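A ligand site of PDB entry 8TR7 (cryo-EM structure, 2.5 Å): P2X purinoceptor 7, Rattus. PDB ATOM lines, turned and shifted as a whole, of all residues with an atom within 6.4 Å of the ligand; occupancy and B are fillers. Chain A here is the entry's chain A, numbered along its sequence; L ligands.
A nitrogen (N3) of the ligand lies within hydrogen-bond range of the backbone carbonyl oxygen of Ala 567, at 3.0 Å.
NH1 of Arg 574 lies within hydrogen-bond range of N2 of the ligand (2.9 Å).
N4 of the ligand sits at hydrogen-bond distance from O of Ala 564 (3.4 Å).
N of Leu 569 is in hydrogen-bond range of O11 of the ligand, at 2.8 Å.
An oxygen (O6) of the ligand is in salt-bridge range of the guanidinium group (NH2) of Arg 578 (3.2 Å).
The side-chain amino group of Lys 583 is in salt-bridge range of an oxygen (O3) of the ligand, 2.4 Å away.
O5 of the ligand is in salt-bridge range of NE of Arg 546 (2.6 Å).
The backbone NH of Gly 590 sits at hydrogen-bond distance from an oxygen (O6) of the ligand.
The backbone NH (N) of Ser 589 sits at hydrogen-bond distance from an oxygen (O3) of the ligand (3.1 Å).
NZ of Lys 592 sits close to OG of Ser 589 (3.3 Å).
The backbone NH of Lys 583 lies within hydrogen-bond range of the side-chain hydroxyl of Tyr 588 (2.7 Å).
The guanidinium group (NE) of Arg 578 is in hydrogen-bond range of the side-chain hydroxyl (OH) of Tyr 550.
The backbone carbonyl oxygen (O) of Ser 543 sits close to a ring nitrogen (NE2) of His 547, at 3.5 Å.
The guanidinium group (NE) of Arg 574 lies within salt-bridge range of the side-chain carboxylate (OE1) of Glu 495 (3.6 Å).
NH1 of Arg 578 lies within salt-bridge range of OE1 of Glu 495 (3.8 Å).
O of Leu 569 sits at hydrogen-bond distance from NH2 of Arg 574, at 2.8 Å.
NZ of Lys 583 is in hydrogen-bond range of O of Gln 587, at 2.7 Å.
Merely in contact with the ligand: Tyr 588, Tyr 550, His 547, Phe 591, Asp 565, Ile 568, Lys 592 and Gln 587.
Hydrophobic or aromatic side chains that line the ligand: His 547, Tyr 550, Leu 569, Tyr 588 and Phe 591.
Within 4 Å of the ligand: Arg 546, His 547, Tyr 550, Ala 564, Asp 565, Ala 567, Ile 568, Leu 569, Arg 574, Arg 578, Lys 583, Gln 587, Tyr 588, Ser 589, Gly 590, Phe 591 and Lys 592.
Along chain A the residues within 4 Å of the ligand span positions 546 to 592.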
ATOM      1  N   GLU A 495     -14.408   8.619 -23.962  1.00  0.00           N
ATOM      2  CA  GLU A 495     -14.855   9.771 -23.189  1.00  0.00           C
ATOM      3  C   GLU A 495     -13.926  10.115 -22.034  1.00  0.00           C
ATOM      4  O   GLU A 495     -14.210  11.063 -21.298  1.00  0.00           O
ATOM      5  CB  GLU A 495     -16.270   9.525 -22.648  1.00  0.00           C
ATOM      6  CG  GLU A 495     -17.315   9.301 -23.716  1.00  0.00           C
ATOM      7  CD  GLU A 495     -18.719   9.564 -23.211  1.00  0.00           C
ATOM      8  OE1 GLU A 495     -18.860   9.994 -22.049  1.00  0.00           O
ATOM      9  OE2 GLU A 495     -19.678   9.366 -23.983  1.00  0.00           O
ATOM     10  N   SER A 543     -32.815  17.750 -25.726  1.00  0.00           N
ATOM     11  CA  SER A 543     -31.821  17.036 -26.503  1.00  0.00           C
ATOM     12  C   SER A 543     -31.222  17.921 -27.590  1.00  0.00           C
ATOM     13  O   SER A 543     -30.014  17.895 -27.840  1.00  0.00           O
ATOM     14  CB  SER A 543     -32.440  15.782 -27.119  1.00  0.00           C
ATOM     15  OG  SER A 543     -33.421  16.123 -28.088  1.00  0.00           O
ATOM     16  N   ARG A 546     -28.788  20.270 -26.004  1.00  0.00           N
ATOM     17  CA  ARG A 546     -27.557  19.561 -25.656  1.00  0.00           C
ATOM     18  C   ARG A 546     -26.681  19.369 -26.887  1.00  0.00           C
ATOM     19  O   ARG A 546     -25.471  19.603 -26.855  1.00  0.00           O
ATOM     20  CB  ARG A 546     -27.916  18.209 -25.024  1.00  0.00           C
ATOM     21  CG  ARG A 546     -26.739  17.441 -24.493  1.00  0.00           C
ATOM     22  CD  ARG A 546     -27.167  16.302 -23.588  1.00  0.00           C
ATOM     23  NE  ARG A 546     -28.160  15.427 -24.189  1.00  0.00           N
ATOM     24  CZ  ARG A 546     -29.464  15.454 -23.927  1.00  0.00           C
ATOM     25  NH1 ARG A 546     -29.969  16.329 -23.074  1.00  0.00           N
ATOM     26  NH2 ARG A 546     -30.276  14.609 -24.538  1.00  0.00           N
ATOM     27  N   HIS A 547     -27.290  18.941 -28.002  1.00  0.00           N
ATOM     28  CA  HIS A 547     -26.537  18.749 -29.233  1.00  0.00           C
ATOM     29  C   HIS A 547     -25.971  20.068 -29.738  1.00  0.00           C
ATOM     30  O   HIS A 547     -24.835  20.116 -30.234  1.00  0.00           O
ATOM     31  CB  HIS A 547     -27.417  18.115 -30.295  1.00  0.00           C
ATOM     32  CG  HIS A 547     -27.992  16.797 -29.885  1.00  0.00           C
ATOM     33  ND1 HIS A 547     -28.862  16.073 -30.687  1.00  0.00           N
ATOM     34  CD2 HIS A 547     -27.834  16.060 -28.766  1.00  0.00           C
ATOM     35  CE1 HIS A 547     -29.200  14.955 -30.077  1.00  0.00           C
ATOM     36  NE2 HIS A 547     -28.595  14.928 -28.904  1.00  0.00           N
ATOM     37  N   TYR A 550     -22.924  20.911 -27.706  1.00  0.00           N
ATOM     38  CA  TYR A 550     -21.786  20.126 -28.201  1.00  0.00           C
ATOM     39  C   TYR A 550     -21.221  20.754 -29.461  1.00  0.00           C
ATOM     40  O   TYR A 550     -19.993  20.938 -29.594  1.00  0.00           O
ATOM     41  CB  TYR A 550     -22.201  18.681 -28.485  1.00  0.00           C
ATOM     42  CG  TYR A 550     -22.659  17.881 -27.285  1.00  0.00           C
ATOM     43  CD1 TYR A 550     -22.187  18.151 -26.011  1.00  0.00           C
ATOM     44  CD2 TYR A 550     -23.542  16.832 -27.435  1.00  0.00           C
ATOM     45  CE1 TYR A 550     -22.602  17.421 -24.931  1.00  0.00           C
ATOM     46  CE2 TYR A 550     -23.964  16.088 -26.362  1.00  0.00           C
ATOM     47  CZ  TYR A 550     -23.491  16.380 -25.114  1.00  0.00           C
ATOM     48  OH  TYR A 550     -23.912  15.636 -24.041  1.00  0.00           O
ATOM     49  N   ALA A 554     -17.507  22.438 -30.119  1.00  0.00           N
ATOM     50  CA  ALA A 554     -16.652  21.862 -31.151  1.00  0.00           C
ATOM     51  C   ALA A 554     -16.276  22.901 -32.189  1.00  0.00           C
ATOM     52  O   ALA A 554     -15.152  22.899 -32.701  1.00  0.00           O
ATOM     53  CB  ALA A 554     -17.358  20.675 -31.801  1.00  0.00           C
ATOM     54  N   MET A 563     -13.086  19.169 -38.850  1.00  0.00           N
ATOM     55  CA  MET A 563     -12.516  18.722 -37.580  1.00  0.00           C
ATOM     56  C   MET A 563     -13.569  18.678 -36.484  1.00  0.00           C
ATOM     57  O   MET A 563     -13.490  17.842 -35.577  1.00  0.00           O
ATOM     58  CB  MET A 563     -11.370  19.641 -37.179  1.00  0.00           C
ATOM     59  CG  MET A 563     -10.138  19.533 -38.055  1.00  0.00           C
ATOM     60  SD  MET A 563      -8.608  19.693 -37.125  1.00  0.00           S
ATOM     61  CE  MET A 563      -8.447  21.470 -37.066  1.00  0.00           C
ATOM     62  N   ALA A 564     -14.561  19.572 -36.546  1.00  0.00           N
ATOM     63  CA  ALA A 564     -15.569  19.627 -35.483  1.00  0.00           C
ATOM     64  C   ALA A 564     -16.448  18.391 -35.485  1.00  0.00           C
ATOM     65  O   ALA A 564     -16.878  17.924 -34.425  1.00  0.00           O
ATOM     66  CB  ALA A 564     -16.423  20.890 -35.662  1.00  0.00           C
ATOM     67  N   ASP A 565     -16.688  17.890 -36.705  1.00  0.00           N
ATOM     68  CA  ASP A 565     -17.526  16.706 -36.817  1.00  0.00           C
ATOM     69  C   ASP A 565     -16.901  15.523 -36.094  1.00  0.00           C
ATOM     70  O   ASP A 565     -17.607  14.713 -35.476  1.00  0.00           O
ATOM     71  CB  ASP A 565     -17.751  16.373 -38.291  1.00  0.00           C
ATOM     72  CG  ASP A 565     -18.500  17.461 -39.024  1.00  0.00           C
ATOM     73  OD1 ASP A 565     -19.200  18.251 -38.352  1.00  0.00           O
ATOM     74  OD2 ASP A 565     -18.384  17.529 -40.260  1.00  0.00           O
ATOM     75  N   PHE A 566     -15.583  15.382 -36.169  1.00  0.00           N
ATOM     76  CA  PHE A 566     -14.868  14.271 -35.567  1.00  0.00           C
ATOM     77  C   PHE A 566     -14.181  14.640 -34.264  1.00  0.00           C
ATOM     78  O   PHE A 566     -13.376  13.865 -33.747  1.00  0.00           O
ATOM     79  CB  PHE A 566     -13.844  13.707 -36.557  1.00  0.00           C
ATOM     80  CG  PHE A 566     -14.468  13.031 -37.726  1.00  0.00           C
ATOM     81  CD1 PHE A 566     -14.781  11.690 -37.685  1.00  0.00           C
ATOM     82  CD2 PHE A 566     -14.752  13.740 -38.882  1.00  0.00           C
ATOM     83  CE1 PHE A 566     -15.364  11.072 -38.764  1.00  0.00           C
ATOM     84  CE2 PHE A 566     -15.339  13.126 -39.954  1.00  0.00           C
ATOM     85  CZ  PHE A 566     -15.638  11.790 -39.896  1.00  0.00           C
ATOM     86  N   ALA A 567     -14.489  15.810 -33.707  1.00  0.00           N
ATOM     87  CA  ALA A 567     -13.914  16.231 -32.454  1.00  0.00           C
ATOM     88  C   ALA A 567     -14.465  15.377 -31.310  1.00  0.00           C
ATOM     89  O   ALA A 567     -15.438  14.643 -31.448  1.00  0.00           O
ATOM     90  CB  ALA A 567     -14.223  17.705 -32.200  1.00  0.00           C
ATOM     91  N   ILE A 568     -13.794  15.467 -30.170  1.00  0.00           N
ATOM     92  CA  ILE A 568     -14.187  14.764 -28.954  1.00  0.00           C
ATOM     93  C   ILE A 568     -14.203  15.767 -27.816  1.00  0.00           C
ATOM     94  O   ILE A 568     -13.208  16.465 -27.582  1.00  0.00           O
ATOM     95  CB  ILE A 568     -13.252  13.590 -28.633  1.00  0.00           C
ATOM     96  CG1 ILE A 568     -13.134  12.643 -29.826  1.00  0.00           C
ATOM     97  CG2 ILE A 568     -13.755  12.829 -27.415  1.00  0.00           C
ATOM     98  CD1 ILE A 568     -14.398  11.909 -30.168  1.00  0.00           C
ATOM     99  N   LEU A 569     -15.328  15.864 -27.132  1.00  0.00           N
ATOM    100  CA  LEU A 569     -15.464  16.812 -26.038  1.00  0.00           C
ATOM    101  C   LEU A 569     -14.798  16.288 -24.774  1.00  0.00           C
ATOM    102  O   LEU A 569     -14.836  15.082 -24.489  1.00  0.00           O
ATOM    103  CB  LEU A 569     -16.931  17.096 -25.769  1.00  0.00           C
ATOM    104  CG  LEU A 569     -17.553  18.275 -26.499  1.00  0.00           C
ATOM    105  CD1 LEU A 569     -17.813  17.949 -27.947  1.00  0.00           C
ATOM    106  CD2 LEU A 569     -18.827  18.657 -25.817  1.00  0.00           C
ATOM    107  N   PRO A 570     -14.192  17.171 -23.975  1.00  0.00           N
ATOM    108  CA  PRO A 570     -13.713  16.762 -22.661  1.00  0.00           C
ATOM    109  C   PRO A 570     -14.845  16.311 -21.764  1.00  0.00           C
ATOM    110  O   PRO A 570     -15.994  16.743 -21.908  1.00  0.00           O
ATOM    111  CB  PRO A 570     -13.023  18.012 -22.120  1.00  0.00           C
ATOM    112  CG  PRO A 570     -12.705  18.820 -23.309  1.00  0.00           C
ATOM    113  CD  PRO A 570     -13.771  18.544 -24.307  1.00  0.00           C
ATOM    114  N   ARG A 574     -18.557  17.992 -21.315  1.00  0.00           N
ATOM    115  CA  ARG A 574     -19.687  17.150 -21.689  1.00  0.00           C
ATOM    116  C   ARG A 574     -20.665  17.000 -20.529  1.00  0.00           C
ATOM    117  O   ARG A 574     -21.878  17.165 -20.692  1.00  0.00           O
ATOM    118  CB  ARG A 574     -19.158  15.783 -22.130  1.00  0.00           C
ATOM    119  CG  ARG A 574     -20.215  14.762 -22.451  1.00  0.00           C
ATOM    120  CD  ARG A 574     -19.617  13.366 -22.483  1.00  0.00           C
ATOM    121  NE  ARG A 574     -18.312  13.354 -23.135  1.00  0.00           N
ATOM    122  CZ  ARG A 574     -18.129  13.315 -24.451  1.00  0.00           C
ATOM    123  NH1 ARG A 574     -19.168  13.282 -25.259  1.00  0.00           N
ATOM    124  NH2 ARG A 574     -16.910  13.313 -24.950  1.00  0.00           N
ATOM    125  N   ARG A 578     -24.506  18.251 -20.064  1.00  0.00           N
ATOM    126  CA  ARG A 578     -25.598  17.315 -19.780  1.00  0.00           C
ATOM    127  C   ARG A 578     -26.331  17.707 -18.501  1.00  0.00           C
ATOM    128  O   ARG A 578     -27.557  17.575 -18.422  1.00  0.00           O
ATOM    129  CB  ARG A 578     -25.042  15.899 -19.683  1.00  0.00           C
ATOM    130  CG  ARG A 578     -24.475  15.397 -20.998  1.00  0.00           C
ATOM    131  CD  ARG A 578     -23.767  14.087 -20.857  1.00  0.00           C
ATOM    132  NE  ARG A 578     -23.592  13.439 -22.155  1.00  0.00           N
ATOM    133  CZ  ARG A 578     -22.775  12.426 -22.383  1.00  0.00           C
ATOM    134  NH1 ARG A 578     -22.046  11.923 -21.403  1.00  0.00           N
ATOM    135  NH2 ARG A 578     -22.683  11.903 -23.593  1.00  0.00           N
ATOM    136  N   LYS A 583     -31.033  14.589 -19.274  1.00  0.00           N
ATOM    137  CA  LYS A 583     -31.818  13.599 -19.990  1.00  0.00           C
ATOM    138  C   LYS A 583     -32.573  12.772 -18.956  1.00  0.00           C
ATOM    139  O   LYS A 583     -31.959  12.112 -18.111  1.00  0.00           O
ATOM    140  CB  LYS A 583     -30.901  12.726 -20.843  1.00  0.00           C
ATOM    141  CG  LYS A 583     -31.568  11.592 -21.579  1.00  0.00           C
ATOM    142  CD  LYS A 583     -30.501  10.698 -22.188  1.00  0.00           C
ATOM    143  CE  LYS A 583     -31.045   9.835 -23.295  1.00  0.00           C
ATOM    144  NZ  LYS A 583     -29.992   8.912 -23.806  1.00  0.00           N
ATOM    145  N   GLY A 586     -32.760   7.125 -19.581  1.00  0.00           N
ATOM    146  CA  GLY A 586     -31.696   6.534 -20.380  1.00  0.00           C
ATOM    147  C   GLY A 586     -30.370   7.221 -20.181  1.00  0.00           C
ATOM    148  O   GLY A 586     -30.286   8.388 -19.784  1.00  0.00           O
ATOM    149  N   GLN A 587     -29.301   6.490 -20.452  1.00  0.00           N
ATOM    150  CA  GLN A 587     -27.962   7.048 -20.400  1.00  0.00           C
ATOM    151  C   GLN A 587     -27.585   7.642 -21.752  1.00  0.00           C
ATOM    152  O   GLN A 587     -28.118   7.256 -22.800  1.00  0.00           O
ATOM    153  CB  GLN A 587     -26.940   5.997 -19.977  1.00  0.00           C
ATOM    154  CG  GLN A 587     -26.804   5.844 -18.471  1.00  0.00           C
ATOM    155  CD  GLN A 587     -25.718   4.871 -18.071  1.00  0.00           C
ATOM    156  OE1 GLN A 587     -25.355   3.984 -18.840  1.00  0.00           O
ATOM    157  NE2 GLN A 587     -25.180   5.048 -16.874  1.00  0.00           N
ATOM    158  N   TYR A 588     -26.647   8.577 -21.723  1.00  0.00           N
ATOM    159  CA  TYR A 588     -26.300   9.332 -22.918  1.00  0.00           C
ATOM    160  C   TYR A 588     -25.548   8.467 -23.913  1.00  0.00           C
ATOM    161  O   TYR A 588     -24.680   7.676 -23.544  1.00  0.00           O
ATOM    162  CB  TYR A 588     -25.480  10.555 -22.547  1.00  0.00           C
ATOM    163  CG  TYR A 588     -26.251  11.549 -21.712  1.00  0.00           C
ATOM    164  CD1 TYR A 588     -27.029  12.519 -22.303  1.00  0.00           C
ATOM    165  CD2 TYR A 588     -26.197  11.502 -20.323  1.00  0.00           C
ATOM    166  CE1 TYR A 588     -27.733  13.428 -21.549  1.00  0.00           C
ATOM    167  CE2 TYR A 588     -26.897  12.407 -19.552  1.00  0.00           C
ATOM    168  CZ  TYR A 588     -27.662  13.372 -20.171  1.00  0.00           C
ATOM    169  OH  TYR A 588     -28.367  14.272 -19.413  1.00  0.00           O
ATOM    170  N   SER A 589     -25.885   8.641 -25.194  1.00  0.00           N
ATOM    171  CA  SER A 589     -25.353   7.769 -26.238  1.00  0.00           C
ATOM    172  C   SER A 589     -23.886   8.070 -26.529  1.00  0.00           C
ATOM    173  O   SER A 589     -23.080   7.144 -26.698  1.00  0.00           O
ATOM    174  CB  SER A 589     -26.191   7.910 -27.498  1.00  0.00           C
ATOM    175  OG  SER A 589     -25.699   7.104 -28.537  1.00  0.00           O
ATOM    176  N   GLY A 590     -23.516   9.337 -26.610  1.00  0.00           N
ATOM    177  CA  GLY A 590     -22.150   9.719 -26.887  1.00  0.00           C
ATOM    178  C   GLY A 590     -21.883   9.961 -28.359  1.00  0.00           C
ATOM    179  O   GLY A 590     -22.782  10.059 -29.194  1.00  0.00           O
ATOM    180  N   PHE A 591     -20.593  10.057 -28.675  1.00  0.00           N
ATOM    181  CA  PHE A 591     -20.167  10.385 -30.025  1.00  0.00           C
ATOM    182  C   PHE A 591     -20.561   9.277 -31.001  1.00  0.00           C
ATOM    183  O   PHE A 591     -20.434   8.086 -30.714  1.00  0.00           O
ATOM    184  CB  PHE A 591     -18.662  10.597 -30.067  1.00  0.00           C
ATOM    185  CG  PHE A 591     -18.130  10.911 -31.429  1.00  0.00           C
ATOM    186  CD1 PHE A 591     -18.624  11.979 -32.155  1.00  0.00           C
ATOM    187  CD2 PHE A 591     -17.127  10.141 -31.991  1.00  0.00           C
ATOM    188  CE1 PHE A 591     -18.142  12.263 -33.412  1.00  0.00           C
ATOM    189  CE2 PHE A 591     -16.645  10.426 -33.248  1.00  0.00           C
ATOM    190  CZ  PHE A 591     -17.159  11.493 -33.959  1.00  0.00           C
ATOM    191  N   LYS A 592     -21.031   9.695 -32.176  1.00  0.00           N
ATOM    192  CA  LYS A 592     -21.466   8.792 -33.229  1.00  0.00           C
ATOM    193  C   LYS A 592     -20.730   9.090 -34.525  1.00  0.00           C
ATOM    194  O   LYS A 592     -20.536  10.251 -34.892  1.00  0.00           O
ATOM    195  CB  LYS A 592     -22.969   8.880 -33.474  1.00  0.00           C
ATOM    196  CG  LYS A 592     -23.797   8.391 -32.307  1.00  0.00           C
ATOM    197  CD  LYS A 592     -23.863   6.879 -32.317  1.00  0.00           C
ATOM    198  CE  LYS A 592     -24.389   6.335 -31.009  1.00  0.00           C
ATOM    199  NZ  LYS A 592     -23.446   5.423 -30.327  1.00  0.00           N
ATOM    200  N   TYR A 593     -20.339   8.032 -35.217  1.00  0.00           N
ATOM    201  CA  TYR A 593     -19.615   8.160 -36.472  1.00  0.00           C
ATOM    202  C   TYR A 593     -20.524   8.761 -37.528  1.00  0.00           C
ATOM    203  O   TYR A 593     -21.582   8.189 -37.830  1.00  0.00           O
ATOM    204  CB  TYR A 593     -19.118   6.787 -36.914  1.00  0.00           C
ATOM    205  CG  TYR A 593     -18.373   6.807 -38.222  1.00  0.00           C
ATOM    206  CD1 TYR A 593     -17.369   7.735 -38.460  1.00  0.00           C
ATOM    207  CD2 TYR A 593     -18.666   5.894 -39.219  1.00  0.00           C
ATOM    208  CE1 TYR A 593     -16.692   7.756 -39.652  1.00  0.00           C
ATOM    209  CE2 TYR A 593     -17.986   5.902 -40.415  1.00  0.00           C
ATOM    210  CZ  TYR A 593     -17.006   6.835 -40.630  1.00  0.00           C
ATOM    211  OH  TYR A 593     -16.320   6.856 -41.817  1.00  0.00           O
HETATM  212  P1  LIG L   1     -28.723  11.255 -26.235  1.00  0.00           P
HETATM  213  O1  LIG L   1     -29.016  12.315 -25.200  1.00  0.00           O
HETATM  214  O2  LIG L   1     -29.798  11.245 -27.291  1.00  0.00           O
HETATM  215  O3  LIG L   1     -28.667   9.894 -25.583  1.00  0.00           O
HETATM  216  O4  LIG L   1     -27.315  11.554 -26.949  1.00  0.00           O
HETATM  217  P2  LIG L   1     -26.209  12.558 -26.364  1.00  0.00           P
HETATM  218  O5  LIG L   1     -26.800  13.571 -25.420  1.00  0.00           O
HETATM  219  O6  LIG L   1     -25.050  11.819 -25.732  1.00  0.00           O
HETATM  220  O7  LIG L   1     -25.742  13.254 -27.728  1.00  0.00           O
HETATM  221  C1  LIG L   1     -25.471  12.410 -28.836  1.00  0.00           C
HETATM  222  C2  LIG L   1     -25.191  13.251 -30.064  1.00  0.00           C
HETATM  223  O8  LIG L   1     -24.238  14.251 -29.710  1.00  0.00           O
HETATM  224  C3  LIG L   1     -24.606  12.407 -31.173  1.00  0.00           C
HETATM  225  O9  LIG L   1     -25.291  12.630 -32.412  1.00  0.00           O
HETATM  226  C4  LIG L   1     -23.148  12.821 -31.279  1.00  0.00           C
HETATM  227  O10 LIG L   1     -22.770  13.022 -32.631  1.00  0.00           O
HETATM  228  C5  LIG L   1     -23.040  14.105 -30.468  1.00  0.00           C
HETATM  229  N1  LIG L   1     -21.883  14.056 -29.550  1.00  0.00           N
HETATM  230  C6  LIG L   1     -21.901  13.612 -28.287  1.00  0.00           C
HETATM  231  N2  LIG L   1     -20.667  13.716 -27.722  1.00  0.00           N
HETATM  232  C7  LIG L   1     -19.849  14.235 -28.646  1.00  0.00           C
HETATM  233  C8  LIG L   1     -18.426  14.604 -28.720  1.00  0.00           C
HETATM  234  O11 LIG L   1     -17.660  14.451 -27.745  1.00  0.00           O
HETATM  235  N3  LIG L   1     -17.967  15.114 -29.866  1.00  0.00           N
HETATM  236  C9  LIG L   1     -18.757  15.295 -30.932  1.00  0.00           C
HETATM  237  N4  LIG L   1     -18.214  15.827 -32.047  1.00  0.00           N
HETATM  238  N5  LIG L   1     -20.075  14.990 -30.942  1.00  0.00           N
HETATM  239  C10 LIG L   1     -20.654  14.455 -29.845  1.00  0.00           C
